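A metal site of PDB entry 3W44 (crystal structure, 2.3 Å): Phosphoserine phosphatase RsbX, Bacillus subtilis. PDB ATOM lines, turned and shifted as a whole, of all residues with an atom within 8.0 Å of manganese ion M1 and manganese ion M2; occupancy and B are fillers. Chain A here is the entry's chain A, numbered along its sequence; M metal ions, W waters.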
ATOM      1  N   LYS A  19      12.488  -5.751 -21.781  1.00  0.00           N
ATOM      2  CA  LYS A  19      11.082  -6.004 -22.023  1.00  0.00           C
ATOM      3  C   LYS A  19      10.475  -6.638 -20.770  1.00  0.00           C
ATOM      4  O   LYS A  19      11.121  -7.417 -20.133  1.00  0.00           O
ATOM      5  CB  LYS A  19      10.960  -6.959 -23.208  1.00  0.00           C
ATOM      6  CG  LYS A  19       9.551  -7.432 -23.473  1.00  0.00           C
ATOM      7  CD  LYS A  19       9.387  -8.174 -24.771  1.00  0.00           C
ATOM      8  CE  LYS A  19       7.895  -8.334 -25.082  1.00  0.00           C
ATOM      9  NZ  LYS A  19       7.671  -9.206 -26.271  1.00  0.00           N
ATOM     10  N   CYS A  25      18.217  -8.665 -21.863  1.00  0.00           N
ATOM     11  CA  CYS A  25      17.881  -7.627 -22.830  1.00  0.00           C
ATOM     12  C   CYS A  25      18.149  -8.109 -24.267  1.00  0.00           C
ATOM     13  O   CYS A  25      19.277  -8.445 -24.595  1.00  0.00           O
ATOM     14  CB  CYS A  25      18.688  -6.346 -22.527  1.00  0.00           C
ATOM     15  SG  CYS A  25      17.846  -4.911 -23.251  1.00  0.00           S
ATOM     16  N   GLY A  26      17.109  -8.149 -25.096  1.00  0.00           N
ATOM     17  CA  GLY A  26      17.305  -8.245 -26.536  1.00  0.00           C
ATOM     18  C   GLY A  26      18.167  -7.147 -27.181  1.00  0.00           C
ATOM     19  O   GLY A  26      18.801  -7.413 -28.203  1.00  0.00           O
ATOM     20  N   ASP A  27      18.209  -5.924 -26.613  1.00  0.00           N
ATOM     21  CA  ASP A  27      19.098  -4.821 -27.080  1.00  0.00           C
ATOM     22  C   ASP A  27      20.495  -4.940 -26.548  1.00  0.00           C
ATOM     23  O   ASP A  27      20.679  -5.488 -25.497  1.00  0.00           O
ATOM     24  CB  ASP A  27      18.582  -3.466 -26.647  1.00  0.00           C
ATOM     25  CG  ASP A  27      17.201  -3.127 -27.247  1.00  0.00           C
ATOM     26  OD1 ASP A  27      16.695  -3.899 -28.080  1.00  0.00           O
ATOM     27  OD2 ASP A  27      16.609  -2.077 -26.868  1.00  0.00           O
ATOM     28  N   ALA A  43      22.354  -1.914 -30.635  1.00  0.00           N
ATOM     29  CA  ALA A  43      21.797  -2.945 -31.497  1.00  0.00           C
ATOM     30  C   ALA A  43      20.542  -3.508 -30.831  1.00  0.00           C
ATOM     31  O   ALA A  43      20.455  -3.577 -29.621  1.00  0.00           O
ATOM     32  CB  ALA A  43      22.811  -4.035 -31.726  1.00  0.00           C
ATOM     33  N   ASP A  44      19.567  -3.858 -31.637  1.00  0.00           N
ATOM     34  CA  ASP A  44      18.325  -4.399 -31.193  1.00  0.00           C
ATOM     35  C   ASP A  44      18.199  -5.762 -31.872  1.00  0.00           C
ATOM     36  O   ASP A  44      17.841  -5.820 -33.040  1.00  0.00           O
ATOM     37  CB  ASP A  44      17.258  -3.466 -31.704  1.00  0.00           C
ATOM     38  CG  ASP A  44      15.871  -3.935 -31.415  1.00  0.00           C
ATOM     39  OD1 ASP A  44      15.758  -5.071 -30.999  1.00  0.00           O
ATOM     40  OD2 ASP A  44      14.891  -3.179 -31.581  1.00  0.00           O
ATOM     41  N   GLY A  45      18.450  -6.849 -31.174  1.00  0.00           N
ATOM     42  CA  GLY A  45      18.267  -8.211 -31.778  1.00  0.00           C
ATOM     43  C   GLY A  45      16.798  -8.402 -32.142  1.00  0.00           C
ATOM     44  O   GLY A  45      15.949  -7.949 -31.394  1.00  0.00           O
ATOM     45  N   LEU A  46      16.509  -9.033 -33.285  1.00  0.00           N
ATOM     46  CA  LEU A  46      15.149  -9.325 -33.720  1.00  0.00           C
ATOM     47  C   LEU A  46      14.375 -10.037 -32.630  1.00  0.00           C
ATOM     48  O   LEU A  46      14.895 -10.995 -32.090  1.00  0.00           O
ATOM     49  CB  LEU A  46      15.127 -10.141 -35.034  1.00  0.00           C
ATOM     50  CG  LEU A  46      14.813  -9.176 -36.192  1.00  0.00           C
ATOM     51  CD1 LEU A  46      15.939  -8.149 -36.343  1.00  0.00           C
ATOM     52  CD2 LEU A  46      14.471  -9.820 -37.584  1.00  0.00           C
ATOM     53  N   GLY A  47      13.176  -9.565 -32.297  1.00  0.00           N
ATOM     54  CA  GLY A  47      12.362 -10.177 -31.274  1.00  0.00           C
ATOM     55  C   GLY A  47      12.923  -9.758 -29.938  1.00  0.00           C
ATOM     56  O   GLY A  47      13.457  -8.638 -29.774  1.00  0.00           O
ATOM     57  N   SER A  48      12.804 -10.629 -28.948  1.00  0.00           N
ATOM     58  CA  SER A  48      13.546 -10.396 -27.695  1.00  0.00           C
ATOM     59  C   SER A  48      13.960 -11.757 -27.094  1.00  0.00           C
ATOM     60  O   SER A  48      13.933 -12.805 -27.776  1.00  0.00           O
ATOM     61  CB  SER A  48      12.751  -9.503 -26.742  1.00  0.00           C
ATOM     62  OG  SER A  48      11.404  -9.954 -26.751  1.00  0.00           O
ATOM     63  N   GLY A  49      14.348 -11.752 -25.828  1.00  0.00           N
ATOM     64  CA  GLY A  49      14.771 -12.961 -25.247  1.00  0.00           C
ATOM     65  C   GLY A  49      16.214 -13.150 -25.582  1.00  0.00           C
ATOM     66  O   GLY A  49      16.928 -12.228 -26.089  1.00  0.00           O
ATOM     67  N   ALA A  52      17.436 -13.017 -29.230  1.00  0.00           N
ATOM     68  CA  ALA A  52      17.624 -11.618 -29.624  1.00  0.00           C
ATOM     69  C   ALA A  52      18.943 -11.072 -29.028  1.00  0.00           C
ATOM     70  O   ALA A  52      19.728 -10.403 -29.695  1.00  0.00           O
ATOM     71  CB  ALA A  52      16.429 -10.753 -29.198  1.00  0.00           C
ATOM     72  N   ASN A  53      19.216 -11.422 -27.792  1.00  0.00           N
ATOM     73  CA  ASN A  53      20.409 -10.972 -27.157  1.00  0.00           C
ATOM     74  C   ASN A  53      21.609 -11.651 -27.728  1.00  0.00           C
ATOM     75  O   ASN A  53      22.666 -11.028 -27.825  1.00  0.00           O
ATOM     76  CB  ASN A  53      20.326 -11.187 -25.656  1.00  0.00           C
ATOM     77  CG  ASN A  53      21.660 -10.931 -24.976  1.00  0.00           C
ATOM     78  OD1 ASN A  53      22.539 -11.778 -25.020  1.00  0.00           O
ATOM     79  ND2 ASN A  53      21.809  -9.756 -24.350  1.00  0.00           N
ATOM     80  N   SER A  56      22.352  -9.375 -30.622  1.00  0.00           N
ATOM     81  CA  SER A  56      22.819  -8.071 -30.221  1.00  0.00           C
ATOM     82  C   SER A  56      24.120  -8.024 -29.404  1.00  0.00           C
ATOM     83  O   SER A  56      24.938  -7.132 -29.620  1.00  0.00           O
ATOM     84  CB  SER A  56      21.699  -7.233 -29.597  1.00  0.00           C
ATOM     85  OG  SER A  56      21.417  -7.732 -28.335  1.00  0.00           O
ATOM     86  N   ARG A  86      19.344 -14.703 -35.288  1.00  0.00           N
ATOM     87  CA  ARG A  86      18.140 -13.952 -35.555  1.00  0.00           C
ATOM     88  C   ARG A  86      18.376 -12.695 -36.389  1.00  0.00           C
ATOM     89  O   ARG A  86      17.501 -12.331 -37.169  1.00  0.00           O
ATOM     90  CB  ARG A  86      17.496 -13.507 -34.278  1.00  0.00           C
ATOM     91  CG  ARG A  86      16.520 -14.534 -33.830  1.00  0.00           C
ATOM     92  CD  ARG A  86      15.407 -13.932 -33.120  1.00  0.00           C
ATOM     93  NE  ARG A  86      14.790 -14.999 -32.361  1.00  0.00           N
ATOM     94  CZ  ARG A  86      14.285 -14.850 -31.138  1.00  0.00           C
ATOM     95  NH1 ARG A  86      14.307 -13.660 -30.533  1.00  0.00           N
ATOM     96  NH2 ARG A  86      13.726 -15.905 -30.548  1.00  0.00           N
ATOM     97  N   GLY A  87      19.530 -12.028 -36.215  1.00  0.00           N
ATOM     98  CA  GLY A  87      19.775 -10.752 -36.895  1.00  0.00           C
ATOM     99  C   GLY A  87      19.452  -9.633 -35.950  1.00  0.00           C
ATOM    100  O   GLY A  87      18.963  -9.863 -34.834  1.00  0.00           O
ATOM    101  N   ALA A  88      19.730  -8.409 -36.360  1.00  0.00           N
ATOM    102  CA  ALA A  88      19.554  -7.274 -35.460  1.00  0.00           C
ATOM    103  C   ALA A  88      19.526  -5.980 -36.273  1.00  0.00           C
ATOM    104  O   ALA A  88      20.066  -5.937 -37.320  1.00  0.00           O
ATOM    105  CB  ALA A  88      20.708  -7.267 -34.496  1.00  0.00           C
ATOM    106  N   THR A  89      18.926  -4.916 -35.740  1.00  0.00           N
ATOM    107  CA  THR A  89      19.131  -3.596 -36.283  1.00  0.00           C
ATOM    108  C   THR A  89      20.225  -2.935 -35.458  1.00  0.00           C
ATOM    109  O   THR A  89      20.402  -3.256 -34.334  1.00  0.00           O
ATOM    110  CB  THR A  89      17.834  -2.830 -36.306  1.00  0.00           C
ATOM    111  OG1 THR A  89      17.287  -2.809 -35.002  1.00  0.00           O
ATOM    112  CG2 THR A  89      16.822  -3.585 -37.219  1.00  0.00           C
ATOM    113  N   ASN A 109      15.819   0.016 -37.981  1.00  0.00           N
ATOM    114  CA  ASN A 109      15.216   1.068 -37.219  1.00  0.00           C
ATOM    115  C   ASN A 109      15.870   1.396 -35.885  1.00  0.00           C
ATOM    116  O   ASN A 109      15.191   1.382 -34.861  1.00  0.00           O
ATOM    117  CB  ASN A 109      13.707   0.795 -37.016  1.00  0.00           C
ATOM    118  CG  ASN A 109      12.943   2.039 -36.548  1.00  0.00           C
ATOM    119  OD1 ASN A 109      13.485   3.123 -36.544  1.00  0.00           O
ATOM    120  ND2 ASN A 109      11.711   1.879 -36.138  1.00  0.00           N
ATOM    121  N   VAL A 110      17.160   1.637 -35.838  1.00  0.00           N
ATOM    122  CA  VAL A 110      17.760   2.252 -34.660  1.00  0.00           C
ATOM    123  C   VAL A 110      18.001   3.707 -35.064  1.00  0.00           C
ATOM    124  O   VAL A 110      18.492   3.947 -36.181  1.00  0.00           O
ATOM    125  CB  VAL A 110      19.046   1.521 -34.221  1.00  0.00           C
ATOM    126  CG1 VAL A 110      19.677   2.217 -32.950  1.00  0.00           C
ATOM    127  CG2 VAL A 110      18.694   0.104 -33.875  1.00  0.00           C
ATOM    128  N   THR A 155      16.936   2.443 -29.631  1.00  0.00           N
ATOM    129  CA  THR A 155      16.152   1.424 -30.241  1.00  0.00           C
ATOM    130  C   THR A 155      14.657   1.795 -30.323  1.00  0.00           C
ATOM    131  O   THR A 155      14.202   2.828 -29.773  1.00  0.00           O
ATOM    132  CB  THR A 155      16.316   0.095 -29.511  1.00  0.00           C
ATOM    133  OG1 THR A 155      15.912   0.285 -28.181  1.00  0.00           O
ATOM    134  CG2 THR A 155      17.735  -0.372 -29.474  1.00  0.00           C
ATOM    135  N   ASP A 156      13.875   0.987 -31.044  1.00  0.00           N
ATOM    136  CA  ASP A 156      12.500   1.335 -31.367  1.00  0.00           C
ATOM    137  C   ASP A 156      11.604   1.148 -30.158  1.00  0.00           C
ATOM    138  O   ASP A 156      10.449   1.507 -30.189  1.00  0.00           O
ATOM    139  CB  ASP A 156      11.970   0.502 -32.537  1.00  0.00           C
ATOM    140  CG  ASP A 156      12.082  -1.017 -32.289  1.00  0.00           C
ATOM    141  OD1 ASP A 156      12.310  -1.467 -31.153  1.00  0.00           O
ATOM    142  OD2 ASP A 156      11.938  -1.773 -33.287  1.00  0.00           O
ATOM    143  N   GLY A 157      12.124   0.598 -29.078  1.00  0.00           N
ATOM    144  CA  GLY A 157      11.376   0.601 -27.817  1.00  0.00           C
ATOM    145  C   GLY A 157      11.070   1.962 -27.191  1.00  0.00           C
ATOM    146  O   GLY A 157      10.196   2.079 -26.307  1.00  0.00           O
ATOM    147  N   LEU A 158      11.809   2.968 -27.598  1.00  0.00           N
ATOM    148  CA  LEU A 158      11.618   4.300 -27.050  1.00  0.00           C
ATOM    149  C   LEU A 158      10.774   4.991 -28.078  1.00  0.00           C
ATOM    150  O   LEU A 158      11.235   5.196 -29.228  1.00  0.00           O
ATOM    151  CB  LEU A 158      12.954   5.045 -26.926  1.00  0.00           C
ATOM    152  CG  LEU A 158      12.895   6.491 -26.432  1.00  0.00           C
ATOM    153  CD1 LEU A 158      12.470   6.523 -24.925  1.00  0.00           C
ATOM    154  CD2 LEU A 158      14.240   7.218 -26.640  1.00  0.00           C
ATOM    155  N   LYS A 188       6.835  -2.567 -23.063  1.00  0.00           N
ATOM    156  CA  LYS A 188       6.300  -3.301 -24.185  1.00  0.00           C
ATOM    157  C   LYS A 188       7.462  -3.933 -24.968  1.00  0.00           C
ATOM    158  O   LYS A 188       7.302  -4.990 -25.590  1.00  0.00           O
ATOM    159  CB  LYS A 188       5.413  -2.418 -25.061  1.00  0.00           C
ATOM    160  CG  LYS A 188       4.135  -1.944 -24.326  1.00  0.00           C
ATOM    161  CD  LYS A 188       2.886  -1.978 -25.199  1.00  0.00           C
ATOM    162  CE  LYS A 188       1.639  -2.234 -24.326  1.00  0.00           C
ATOM    163  NZ  LYS A 188       1.787  -3.451 -23.415  1.00  0.00           N
ATOM    164  N   ASP A 189       8.660  -3.339 -24.885  1.00  0.00           N
ATOM    165  CA  ASP A 189       9.790  -3.844 -25.645  1.00  0.00           C
ATOM    166  C   ASP A 189      11.029  -3.531 -24.847  1.00  0.00           C
ATOM    167  O   ASP A 189      10.951  -2.769 -23.938  1.00  0.00           O
ATOM    168  CB  ASP A 189       9.798  -3.136 -26.995  1.00  0.00           C
ATOM    169  CG  ASP A 189      10.843  -3.653 -27.963  1.00  0.00           C
ATOM    170  OD1 ASP A 189      11.476  -4.714 -27.778  1.00  0.00           O
ATOM    171  OD2 ASP A 189      11.029  -2.958 -28.948  1.00  0.00           O
ATOM    172  N   ASP A 190      12.156  -4.129 -25.194  1.00  0.00           N
ATOM    173  CA  ASP A 190      13.419  -3.719 -24.680  1.00  0.00           C
ATOM    174  C   ASP A 190      13.611  -2.260 -25.094  1.00  0.00           C
ATOM    175  O   ASP A 190      13.187  -1.884 -26.169  1.00  0.00           O
ATOM    176  CB  ASP A 190      14.566  -4.563 -25.289  1.00  0.00           C
ATOM    177  CG  ASP A 190      14.470  -6.046 -24.961  1.00  0.00           C
ATOM    178  OD1 ASP A 190      14.395  -6.414 -23.787  1.00  0.00           O
ATOM    179  OD2 ASP A 190      14.535  -6.879 -25.886  1.00  0.00           O
ATOM    180  N   LEU A 191      14.328  -1.481 -24.309  1.00  0.00           N
ATOM    181  CA  LEU A 191      14.459  -0.063 -24.544  1.00  0.00           C
ATOM    182  C   LEU A 191      15.858   0.366 -24.212  1.00  0.00           C
ATOM    183  O   LEU A 191      16.270   0.236 -23.110  1.00  0.00           O
ATOM    184  CB  LEU A 191      13.404   0.718 -23.721  1.00  0.00           C
ATOM    185  CG  LEU A 191      13.116   2.184 -24.105  1.00  0.00           C
ATOM    186  CD1 LEU A 191      11.987   2.655 -23.392  1.00  0.00           C
ATOM    187  CD2 LEU A 191      14.195   3.117 -23.753  1.00  0.00           C
ATOM    188  N   THR A 192      16.605   0.854 -25.197  1.00  0.00           N
ATOM    189  CA  THR A 192      18.000   1.264 -24.998  1.00  0.00           C
ATOM    190  C   THR A 192      18.175   2.617 -25.630  1.00  0.00           C
ATOM    191  O   THR A 192      17.748   2.812 -26.760  1.00  0.00           O
ATOM    192  CB  THR A 192      18.923   0.312 -25.698  1.00  0.00           C
ATOM    193  OG1 THR A 192      18.764  -0.945 -25.117  1.00  0.00           O
ATOM    194  CG2 THR A 192      20.405   0.688 -25.606  1.00  0.00           C
HETATM  195 MN    MN M   1      12.893  -3.342 -30.335  1.00  0.00          MN
HETATM  196 MN    MN M   2      14.469  -6.737 -30.406  1.00  0.00          MN
HETATM  197  O   HOH W   1      12.023  -4.262 -32.307  1.00  0.00           O
HETATM  198  O   HOH W   2      13.438  -6.497 -32.446  1.00  0.00           O
HETATM  199  O   HOH W   3      12.879  -5.580 -29.866  1.00  0.00           O
HETATM  200  O   HOH W   4      15.570  -6.306 -28.480  1.00  0.00           O
HETATM  201  O   HOH W   5      14.346  -2.987 -28.594  1.00  0.00           O
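O of Gly 26 sits at hydrogen-bond distance from N of Gly 45. O of Thr 89 sits at hydrogen-bond distance from N of Asp 44 (2.9 Å). NH1 of Arg 86 is in hydrogen-bond range of O of Leu 46, 3.1 Å away. The backbone NH (N) of Leu 46 sits at hydrogen-bond distance from the backbone carbonyl oxygen (O) of Gly 87 (3.0 Å).
Of the 29 residues printed, 3 come within 4 Å of manganese ion M1.
Merely in contact with manganese ion M2: Leu 46. Within 4 Å of manganese ion M2: Asp 44, Gly 45, Leu 46 and Gly 47. The nearest printed residue that does not touch manganese ion M2 is Asp 27 (4.3 Å).
Manganese ion M1 is bound by the side-chain carboxylate (OD1) of Asp 156 (2.1 Å), water W3 (2.3 Å), water W5 (2.3 Å), water W1 (2.3 Å), the side-chain carboxylate (OD2) of Asp 189 (2.4 Å) and the side-chain carboxylate (OD2) of Asp 44 (2.4 Å). Manganese ion M1 has six donor atoms within binding distance.
Water W3 binds manganese ion M2 (2.0 Å). Manganese ion M2 is bound by O of Gly 45 (2.2 Å). The side-chain carboxylate (OD1) of Asp 44 binds manganese ion M2, 2.2 Å away. The backbone carbonyl oxygen (O) of Gly 47 binds manganese ion M2 (2.2 Å). Water W4 binds manganese ion M2 (2.3 Å). Water W2 is bound to manganese ion M2 (2.3 Å).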
